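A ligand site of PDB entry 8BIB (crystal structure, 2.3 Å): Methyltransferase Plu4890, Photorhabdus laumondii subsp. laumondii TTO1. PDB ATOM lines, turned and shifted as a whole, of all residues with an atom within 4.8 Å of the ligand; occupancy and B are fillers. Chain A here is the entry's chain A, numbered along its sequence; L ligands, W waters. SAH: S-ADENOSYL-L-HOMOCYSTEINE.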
ATOM      1  N   PHE A 127      -4.673   5.290  22.131  1.00  0.00           N
ATOM      2  CA  PHE A 127      -5.724   5.636  23.130  1.00  0.00           C
ATOM      3  C   PHE A 127      -5.562   4.799  24.399  1.00  0.00           C
ATOM      4  O   PHE A 127      -5.834   5.338  25.488  1.00  0.00           O
ATOM      5  CB  PHE A 127      -7.116   5.489  22.503  1.00  0.00           C
ATOM      6  CG  PHE A 127      -7.414   6.501  21.433  1.00  0.00           C
ATOM      7  CD1 PHE A 127      -7.401   7.859  21.728  1.00  0.00           C
ATOM      8  CD2 PHE A 127      -7.702   6.115  20.135  1.00  0.00           C
ATOM      9  CE1 PHE A 127      -7.666   8.805  20.740  1.00  0.00           C
ATOM     10  CE2 PHE A 127      -7.965   7.055  19.155  1.00  0.00           C
ATOM     11  CZ  PHE A 127      -7.955   8.390  19.458  1.00  0.00           C
ATOM     12  N   PHE A 140      -3.988  16.071  24.508  1.00  0.00           N
ATOM     13  CA  PHE A 140      -4.780  15.550  23.359  1.00  0.00           C
ATOM     14  C   PHE A 140      -6.250  15.938  23.551  1.00  0.00           C
ATOM     15  O   PHE A 140      -6.826  16.557  22.629  1.00  0.00           O
ATOM     16  CB  PHE A 140      -4.636  14.039  23.212  1.00  0.00           C
ATOM     17  CG  PHE A 140      -5.371  13.475  22.024  1.00  0.00           C
ATOM     18  CD1 PHE A 140      -4.757  13.420  20.777  1.00  0.00           C
ATOM     19  CD2 PHE A 140      -6.676  13.023  22.132  1.00  0.00           C
ATOM     20  CE1 PHE A 140      -5.438  12.910  19.673  1.00  0.00           C
ATOM     21  CE2 PHE A 140      -7.350  12.524  21.035  1.00  0.00           C
ATOM     22  CZ  PHE A 140      -6.725  12.466  19.809  1.00  0.00           C
ATOM     23  N   ASP A 141      -6.830  15.564  24.695  1.00  0.00           N
ATOM     24  CA  ASP A 141      -8.251  15.837  25.043  1.00  0.00           C
ATOM     25  C   ASP A 141      -8.509  17.343  25.017  1.00  0.00           C
ATOM     26  O   ASP A 141      -9.606  17.744  24.567  1.00  0.00           O
ATOM     27  CB  ASP A 141      -8.622  15.220  26.405  1.00  0.00           C
ATOM     28  CG  ASP A 141      -8.699  13.701  26.394  1.00  0.00           C
ATOM     29  OD1 ASP A 141      -8.663  13.109  25.287  1.00  0.00           O
ATOM     30  OD2 ASP A 141      -8.791  13.110  27.486  1.00  0.00           O
ATOM     31  N   MET A 144      -8.565  18.467  21.249  1.00  0.00           N
ATOM     32  CA  MET A 144      -9.872  18.009  20.698  1.00  0.00           C
ATOM     33  C   MET A 144     -10.993  18.941  21.167  1.00  0.00           C
ATOM     34  O   MET A 144     -11.922  19.198  20.375  1.00  0.00           O
ATOM     35  CB  MET A 144     -10.204  16.573  21.135  1.00  0.00           C
ATOM     36  CG  MET A 144      -9.299  15.506  20.532  1.00  0.00           C
ATOM     37  SD  MET A 144      -8.996  15.691  18.760  1.00  0.00           S
ATOM     38  CE  MET A 144      -7.334  16.358  18.799  1.00  0.00           C
ATOM     39  N   THR A 145     -10.918  19.423  22.418  1.00  0.00           N
ATOM     40  CA  THR A 145     -11.917  20.332  23.048  1.00  0.00           C
ATOM     41  C   THR A 145     -11.896  21.696  22.344  1.00  0.00           C
ATOM     42  O   THR A 145     -12.989  22.230  22.071  1.00  0.00           O
ATOM     43  CB  THR A 145     -11.682  20.466  24.564  1.00  0.00           C
ATOM     44  OG1 THR A 145     -12.292  19.336  25.189  1.00  0.00           O
ATOM     45  CG2 THR A 145     -12.246  21.740  25.137  1.00  0.00           C
ATOM     46  N   VAL A 147     -10.743  22.608  19.259  1.00  0.00           N
ATOM     47  CA  VAL A 147     -11.190  22.503  17.828  1.00  0.00           C
ATOM     48  C   VAL A 147     -12.699  22.248  17.799  1.00  0.00           C
ATOM     49  O   VAL A 147     -13.355  22.733  16.854  1.00  0.00           O
ATOM     50  CB  VAL A 147     -10.411  21.438  17.023  1.00  0.00           C
ATOM     51  CG1 VAL A 147      -8.940  21.811  16.882  1.00  0.00           C
ATOM     52  CG2 VAL A 147     -10.556  20.039  17.599  1.00  0.00           C
ATOM     53  N   SER A 148     -13.239  21.518  18.780  1.00  0.00           N
ATOM     54  CA  SER A 148     -14.701  21.303  18.983  1.00  0.00           C
ATOM     55  C   SER A 148     -15.372  22.649  19.273  1.00  0.00           C
ATOM     56  O   SER A 148     -16.460  22.903  18.710  1.00  0.00           O
ATOM     57  CB  SER A 148     -14.970  20.306  20.078  1.00  0.00           C
ATOM     58  OG  SER A 148     -14.486  19.011  19.724  1.00  0.00           O
ATOM     59  N   GLY A 171     -17.740   9.040  20.778  1.00  0.00           N
ATOM     60  CA  GLY A 171     -16.320   9.462  20.866  1.00  0.00           C
ATOM     61  C   GLY A 171     -16.199  10.970  21.043  1.00  0.00           C
ATOM     62  O   GLY A 171     -15.353  11.571  20.361  1.00  0.00           O
ATOM     63  N   GLY A 172     -17.000  11.545  21.937  1.00  0.00           N
ATOM     64  CA  GLY A 172     -17.125  12.999  22.138  1.00  0.00           C
ATOM     65  C   GLY A 172     -16.017  13.595  22.994  1.00  0.00           C
ATOM     66  O   GLY A 172     -15.949  14.832  23.091  1.00  0.00           O
ATOM     67  N   GLY A 173     -15.186  12.738  23.603  1.00  0.00           N
ATOM     68  CA  GLY A 173     -14.029  13.162  24.435  1.00  0.00           C
ATOM     69  C   GLY A 173     -14.485  13.771  25.742  1.00  0.00           C
ATOM     70  O   GLY A 173     -15.199  13.093  26.495  1.00  0.00           O
ATOM     71  N   LEU A 193     -20.684   9.489  24.572  1.00  0.00           N
ATOM     72  CA  LEU A 193     -20.043   8.153  24.713  1.00  0.00           C
ATOM     73  C   LEU A 193     -18.548   8.276  24.410  1.00  0.00           C
ATOM     74  O   LEU A 193     -18.196   8.909  23.386  1.00  0.00           O
ATOM     75  CB  LEU A 193     -20.714   7.155  23.771  1.00  0.00           C
ATOM     76  CG  LEU A 193     -20.273   5.693  23.942  1.00  0.00           C
ATOM     77  CD1 LEU A 193     -21.431   4.737  23.706  1.00  0.00           C
ATOM     78  CD2 LEU A 193     -19.109   5.354  23.023  1.00  0.00           C
ATOM     79  N   ASP A 194     -17.708   7.693  25.273  1.00  0.00           N
ATOM     80  CA  ASP A 194     -16.228   7.640  25.106  1.00  0.00           C
ATOM     81  C   ASP A 194     -15.682   6.587  26.072  1.00  0.00           C
ATOM     82  O   ASP A 194     -16.495   5.921  26.744  1.00  0.00           O
ATOM     83  CB  ASP A 194     -15.594   9.013  25.333  1.00  0.00           C
ATOM     84  CG  ASP A 194     -14.352   9.268  24.490  1.00  0.00           C
ATOM     85  OD1 ASP A 194     -13.333   8.611  24.761  1.00  0.00           O
ATOM     86  OD2 ASP A 194     -14.422  10.107  23.571  1.00  0.00           O
ATOM     87  N   ARG A 195     -14.356   6.426  26.126  1.00  0.00           N
ATOM     88  CA  ARG A 195     -13.653   5.531  27.074  1.00  0.00           C
ATOM     89  C   ARG A 195     -13.289   6.338  28.329  1.00  0.00           C
ATOM     90  O   ARG A 195     -12.321   7.119  28.272  1.00  0.00           O
ATOM     91  CB  ARG A 195     -12.409   4.922  26.413  1.00  0.00           C
ATOM     92  CG  ARG A 195     -12.743   4.025  25.220  1.00  0.00           C
ATOM     93  CD  ARG A 195     -11.502   3.551  24.474  1.00  0.00           C
ATOM     94  NE  ARG A 195     -10.682   2.658  25.283  1.00  0.00           N
ATOM     95  CZ  ARG A 195      -9.628   3.018  26.023  1.00  0.00           C
ATOM     96  NH1 ARG A 195      -9.253   4.284  26.085  1.00  0.00           N
ATOM     97  NH2 ARG A 195      -8.970   2.105  26.701  1.00  0.00           N
ATOM     98  N   GLY A 210     -18.129   3.356  27.227  1.00  0.00           N
ATOM     99  CA  GLY A 210     -18.436   2.314  26.212  1.00  0.00           C
ATOM    100  C   GLY A 210     -17.331   2.180  25.175  1.00  0.00           C
ATOM    101  O   GLY A 210     -16.260   2.780  25.364  1.00  0.00           O
ATOM    102  N   ASN A 211     -17.616   1.413  24.117  1.00  0.00           N
ATOM    103  CA  ASN A 211     -16.678   1.060  23.023  1.00  0.00           C
ATOM    104  C   ASN A 211     -17.469   0.964  21.723  1.00  0.00           C
ATOM    105  O   ASN A 211     -18.287   0.029  21.609  1.00  0.00           O
ATOM    106  CB  ASN A 211     -15.928  -0.228  23.335  1.00  0.00           C
ATOM    107  CG  ASN A 211     -14.829  -0.563  22.343  1.00  0.00           C
ATOM    108  OD1 ASN A 211     -14.649   0.139  21.346  1.00  0.00           O
ATOM    109  ND2 ASN A 211     -14.092  -1.626  22.607  1.00  0.00           N
ATOM    110  N   PHE A 212     -17.238   1.882  20.773  1.00  0.00           N
ATOM    111  CA  PHE A 212     -18.009   1.975  19.492  1.00  0.00           C
ATOM    112  C   PHE A 212     -17.613   0.829  18.553  1.00  0.00           C
ATOM    113  O   PHE A 212     -18.355   0.585  17.581  1.00  0.00           O
ATOM    114  CB  PHE A 212     -17.876   3.350  18.832  1.00  0.00           C
ATOM    115  CG  PHE A 212     -16.492   3.941  18.712  1.00  0.00           C
ATOM    116  CD1 PHE A 212     -16.234   5.229  19.159  1.00  0.00           C
ATOM    117  CD2 PHE A 212     -15.448   3.237  18.108  1.00  0.00           C
ATOM    118  CE1 PHE A 212     -14.967   5.793  19.023  1.00  0.00           C
ATOM    119  CE2 PHE A 212     -14.191   3.798  17.986  1.00  0.00           C
ATOM    120  CZ  PHE A 212     -13.950   5.073  18.440  1.00  0.00           C
ATOM    121  N   LEU A 213     -16.491   0.148  18.813  1.00  0.00           N
ATOM    122  CA  LEU A 213     -16.071  -1.073  18.085  1.00  0.00           C
ATOM    123  C   LEU A 213     -17.019  -2.225  18.453  1.00  0.00           C
ATOM    124  O   LEU A 213     -17.319  -3.046  17.555  1.00  0.00           O
ATOM    125  CB  LEU A 213     -14.626  -1.435  18.444  1.00  0.00           C
ATOM    126  CG  LEU A 213     -13.562  -0.374  18.140  1.00  0.00           C
ATOM    127  CD1 LEU A 213     -12.210  -0.809  18.677  1.00  0.00           C
ATOM    128  CD2 LEU A 213     -13.489  -0.085  16.653  1.00  0.00           C
ATOM    129  N   LYS A 226     -17.630  13.032  15.256  1.00  0.00           N
ATOM    130  CA  LYS A 226     -16.691  14.092  14.800  1.00  0.00           C
ATOM    131  C   LYS A 226     -15.236  13.644  15.044  1.00  0.00           C
ATOM    132  O   LYS A 226     -14.899  13.341  16.204  1.00  0.00           O
ATOM    133  CB  LYS A 226     -16.980  15.424  15.506  1.00  0.00           C
ATOM    134  CG  LYS A 226     -16.445  16.650  14.781  1.00  0.00           C
ATOM    135  CD  LYS A 226     -16.941  17.975  15.325  1.00  0.00           C
ATOM    136  CE  LYS A 226     -15.946  18.683  16.200  1.00  0.00           C
ATOM    137  NZ  LYS A 226     -15.599  17.891  17.401  1.00  0.00           N
ATOM    138  N   ASN A 227     -14.441  13.610  13.977  1.00  0.00           N
ATOM    139  CA  ASN A 227     -12.967  13.357  14.005  1.00  0.00           C
ATOM    140  C   ASN A 227     -12.676  12.036  14.738  1.00  0.00           C
ATOM    141  O   ASN A 227     -11.820  12.047  15.654  1.00  0.00           O
ATOM    142  CB  ASN A 227     -12.215  14.528  14.643  1.00  0.00           C
ATOM    143  CG  ASN A 227     -12.336  15.815  13.861  1.00  0.00           C
ATOM    144  OD1 ASN A 227     -12.426  15.802  12.633  1.00  0.00           O
ATOM    145  ND2 ASN A 227     -12.340  16.938  14.550  1.00  0.00           N
ATOM    146  N   VAL A 228     -13.354  10.952  14.352  1.00  0.00           N
ATOM    147  CA  VAL A 228     -13.128   9.582  14.901  1.00  0.00           C
ATOM    148  C   VAL A 228     -12.523   8.692  13.799  1.00  0.00           C
ATOM    149  O   VAL A 228     -11.427   8.149  14.023  1.00  0.00           O
ATOM    150  CB  VAL A 228     -14.419   8.954  15.473  1.00  0.00           C
ATOM    151  CG1 VAL A 228     -14.221   7.514  15.904  1.00  0.00           C
ATOM    152  CG2 VAL A 228     -14.983   9.786  16.622  1.00  0.00           C
ATOM    153  N   ASN A 231      -8.910   8.098  12.752  1.00  0.00           N
ATOM    154  CA  ASN A 231      -8.073   7.365  13.744  1.00  0.00           C
ATOM    155  C   ASN A 231      -8.213   5.850  13.554  1.00  0.00           C
ATOM    156  O   ASN A 231      -7.752   5.108  14.443  1.00  0.00           O
ATOM    157  CB  ASN A 231      -8.443   7.720  15.188  1.00  0.00           C
ATOM    158  CG  ASN A 231      -8.433   9.211  15.475  1.00  0.00           C
ATOM    159  OD1 ASN A 231      -7.659   9.958  14.882  1.00  0.00           O
ATOM    160  ND2 ASN A 231      -9.278   9.638  16.391  1.00  0.00           N
ATOM    161  N   TRP A 232      -8.834   5.384  12.456  1.00  0.00           N
ATOM    162  CA  TRP A 232      -9.116   3.944  12.208  1.00  0.00           C
ATOM    163  C   TRP A 232      -8.858   3.578  10.733  1.00  0.00           C
ATOM    164  O   TRP A 232      -8.878   4.483   9.883  1.00  0.00           O
ATOM    165  CB  TRP A 232     -10.544   3.596  12.611  1.00  0.00           C
ATOM    166  CG  TRP A 232     -10.848   3.883  14.046  1.00  0.00           C
ATOM    167  CD1 TRP A 232     -11.574   4.923  14.535  1.00  0.00           C
ATOM    168  CD2 TRP A 232     -10.407   3.127  15.184  1.00  0.00           C
ATOM    169  NE1 TRP A 232     -11.621   4.868  15.904  1.00  0.00           N
ATOM    170  CE2 TRP A 232     -10.920   3.781  16.331  1.00  0.00           C
ATOM    171  CE3 TRP A 232      -9.638   1.973  15.361  1.00  0.00           C
ATOM    172  CZ2 TRP A 232     -10.682   3.302  17.625  1.00  0.00           C
ATOM    173  CZ3 TRP A 232      -9.411   1.497  16.634  1.00  0.00           C
ATOM    174  CH2 TRP A 232      -9.928   2.162  17.751  1.00  0.00           C
HETATM  175  N   SAH L   1     -15.104  13.734  18.861  1.00  0.00           N
HETATM  176  CA  SAH L   1     -14.069  14.515  19.599  1.00  0.00           C
HETATM  177  CB  SAH L   1     -12.808  13.678  19.851  1.00  0.00           C
HETATM  178  CG  SAH L   1     -12.178  13.088  18.605  1.00  0.00           C
HETATM  179  SD  SAH L   1     -10.637  12.204  18.939  1.00  0.00           S
HETATM  180  C   SAH L   1     -13.689  15.762  18.777  1.00  0.00           C
HETATM  181  O   SAH L   1     -13.088  16.701  19.288  1.00  0.00           O
HETATM  182  OXT SAH L   1     -13.979  15.840  17.588  1.00  0.00           O
HETATM  183  C5' SAH L   1     -11.193  10.478  18.996  1.00  0.00           C
HETATM  184  C4' SAH L   1     -11.955  10.139  20.261  1.00  0.00           C
HETATM  185  O4' SAH L   1     -12.435   8.776  20.187  1.00  0.00           O
HETATM  186  C3' SAH L   1     -11.136  10.243  21.547  1.00  0.00           C
HETATM  187  O3' SAH L   1     -11.803  11.071  22.495  1.00  0.00           O
HETATM  188  C2' SAH L   1     -11.031   8.797  22.040  1.00  0.00           C
HETATM  189  O2' SAH L   1     -11.000   8.696  23.442  1.00  0.00           O
HETATM  190  C1' SAH L   1     -12.310   8.197  21.455  1.00  0.00           C
HETATM  191  N9  SAH L   1     -12.260   6.742  21.302  1.00  0.00           N
HETATM  192  C8  SAH L   1     -11.228   6.009  20.784  1.00  0.00           C
HETATM  193  N7  SAH L   1     -11.468   4.717  20.755  1.00  0.00           N
HETATM  194  C5  SAH L   1     -12.734   4.599  21.292  1.00  0.00           C
HETATM  195  C6  SAH L   1     -13.556   3.482  21.521  1.00  0.00           C
HETATM  196  N6  SAH L   1     -13.203   2.229  21.238  1.00  0.00           N
HETATM  197  N1  SAH L   1     -14.780   3.701  22.062  1.00  0.00           N
HETATM  198  C2  SAH L   1     -15.137   4.967  22.344  1.00  0.00           C
HETATM  199  N3  SAH L   1     -14.446   6.094  22.160  1.00  0.00           N
HETATM  200  C4  SAH L   1     -13.243   5.846  21.627  1.00  0.00           C
HETATM  201  O   HOH W   1      -9.418   6.901  24.896  1.00  0.00           O
HETATM  202  O   HOH W   2     -10.780  13.498  23.377  1.00  0.00           O
HETATM  203  O   HOH W   3      -8.702  12.734  16.557  1.00  0.00           O
HETATM  204  O   HOH W   4     -13.481  16.843  21.975  1.00  0.00           O
HETATM  205  O   HOH W   5     -17.059  15.695  19.427  1.00  0.00           O
HETATM  206  O   HOH W   6     -17.732  12.571  18.183  1.00  0.00           O
HETATM  207  O   HOH W   7     -11.095   7.577  17.655  1.00  0.00           O
HETATM  208  O   HOH W   8      -8.807   9.567  24.824  1.00  0.00           O
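The backbone carbonyl oxygen of Asn 227 lies close to a sulfur (SD) of the ligand (3.5 Å).
CD2 of Phe 127 touches C8 of the ligand, at 3.6 Å.
Phe 140 touches the ligand (CE2 to SD, 3.9 Å).
Gly 172 touches the ligand.
Gly 173 touches the ligand.
Arg 195 touches the ligand.
Gly 210 touches the ligand.
Asn 231 touches the ligand (ND2 to C5', 3.3 Å).
CZ2 of Trp 232 touches N7 of the ligand, 3.5 Å away.
Within 4 Å of the ligand: Phe 127, Phe 140, Met 144, Ser 148, Gly 171, Gly 172, Gly 173, Asp 194, Arg 195, Gly 210, Asn 211, Phe 212, Lys 226, Asn 227, Asn 231 and Trp 232.
Water W4 lies within hydrogen-bond range of O of the ligand, O of Met 144, OG of Ser 148 and O of Gly 172.
Water W2 lies within hydrogen-bond range of an oxygen (O3') of the ligand and the side-chain carboxylate of Asp 141.
Water W1 lies within hydrogen-bond range of O2' of the ligand and NH1 of Arg 195.
Water W5 lies within hydrogen-bond range of N of the ligand (2.8 Å) and NZ of Lys 226 (3.3 Å).
Water W6 lies within hydrogen-bond range of a nitrogen (N) of the ligand, the backbone NH (N) of Lys 226 and the backbone carbonyl oxygen (O) of Gly 171.
Water W7 lies within hydrogen-bond range of the side-chain amide nitrogen of Asn 231 (3.0 Å), an oxygen (O4') of the ligand (3.1 Å) and the indole nitrogen of Trp 232 (3.3 Å).
The backbone NH (N) of Leu 213 is in hydrogen-bond range of the side-chain amide oxygen (OD1) of Asn 211, 3.1 Å away.
The side-chain hydroxyl (OG) of Ser 148 is in hydrogen-bond range of the side-chain amino group (NZ) of Lys 226, at 2.8 Å.
N of Gly 171 lies within hydrogen-bond range of O of Leu 193.
OD2 of Asp 194 lies within hydrogen-bond range of N of Gly 173, 2.7 Å away.
The backbone carbonyl oxygen (O) of Asp 194 is in hydrogen-bond range of the backbone NH (N) of Gly 210 (3.1 Å).
The side-chain carboxylate of Asp 194 is in hydrogen-bond range of the backbone NH of Gly 172 (3.4 Å).
OG of Ser 148 lies within hydrogen-bond range of O of Met 144.
The backbone NH (N) of Gly 172 sits at hydrogen-bond distance from the backbone carbonyl oxygen (O) of Leu 193, 3.2 Å away.
N6 of the ligand is in hydrogen-bond range of OD1 of Asn 211 (2.5 Å).
The backbone carbonyl oxygen (O) of Lys 226 sits at hydrogen-bond distance from a nitrogen (N) of the ligand, 2.7 Å away.
The side-chain amino group (NZ) of Lys 226 is in salt-bridge range of an oxygen (OXT) of the ligand.
A nitrogen (N) of the ligand sits at hydrogen-bond distance from the backbone carbonyl oxygen of Gly 171 (2.6 Å).
O2' of the ligand sits at hydrogen-bond distance from OD1 of Asp 194.
OG of Ser 148 sits at hydrogen-bond distance from O of the ligand (2.7 Å).
The backbone carbonyl oxygen (O) of Met 144 sits close to an oxygen (O) of the ligand, 3.0 Å away.
The backbone NH (N) of Phe 212 lies within hydrogen-bond range of a nitrogen (N1) of the ligand, at 3.3 Å.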
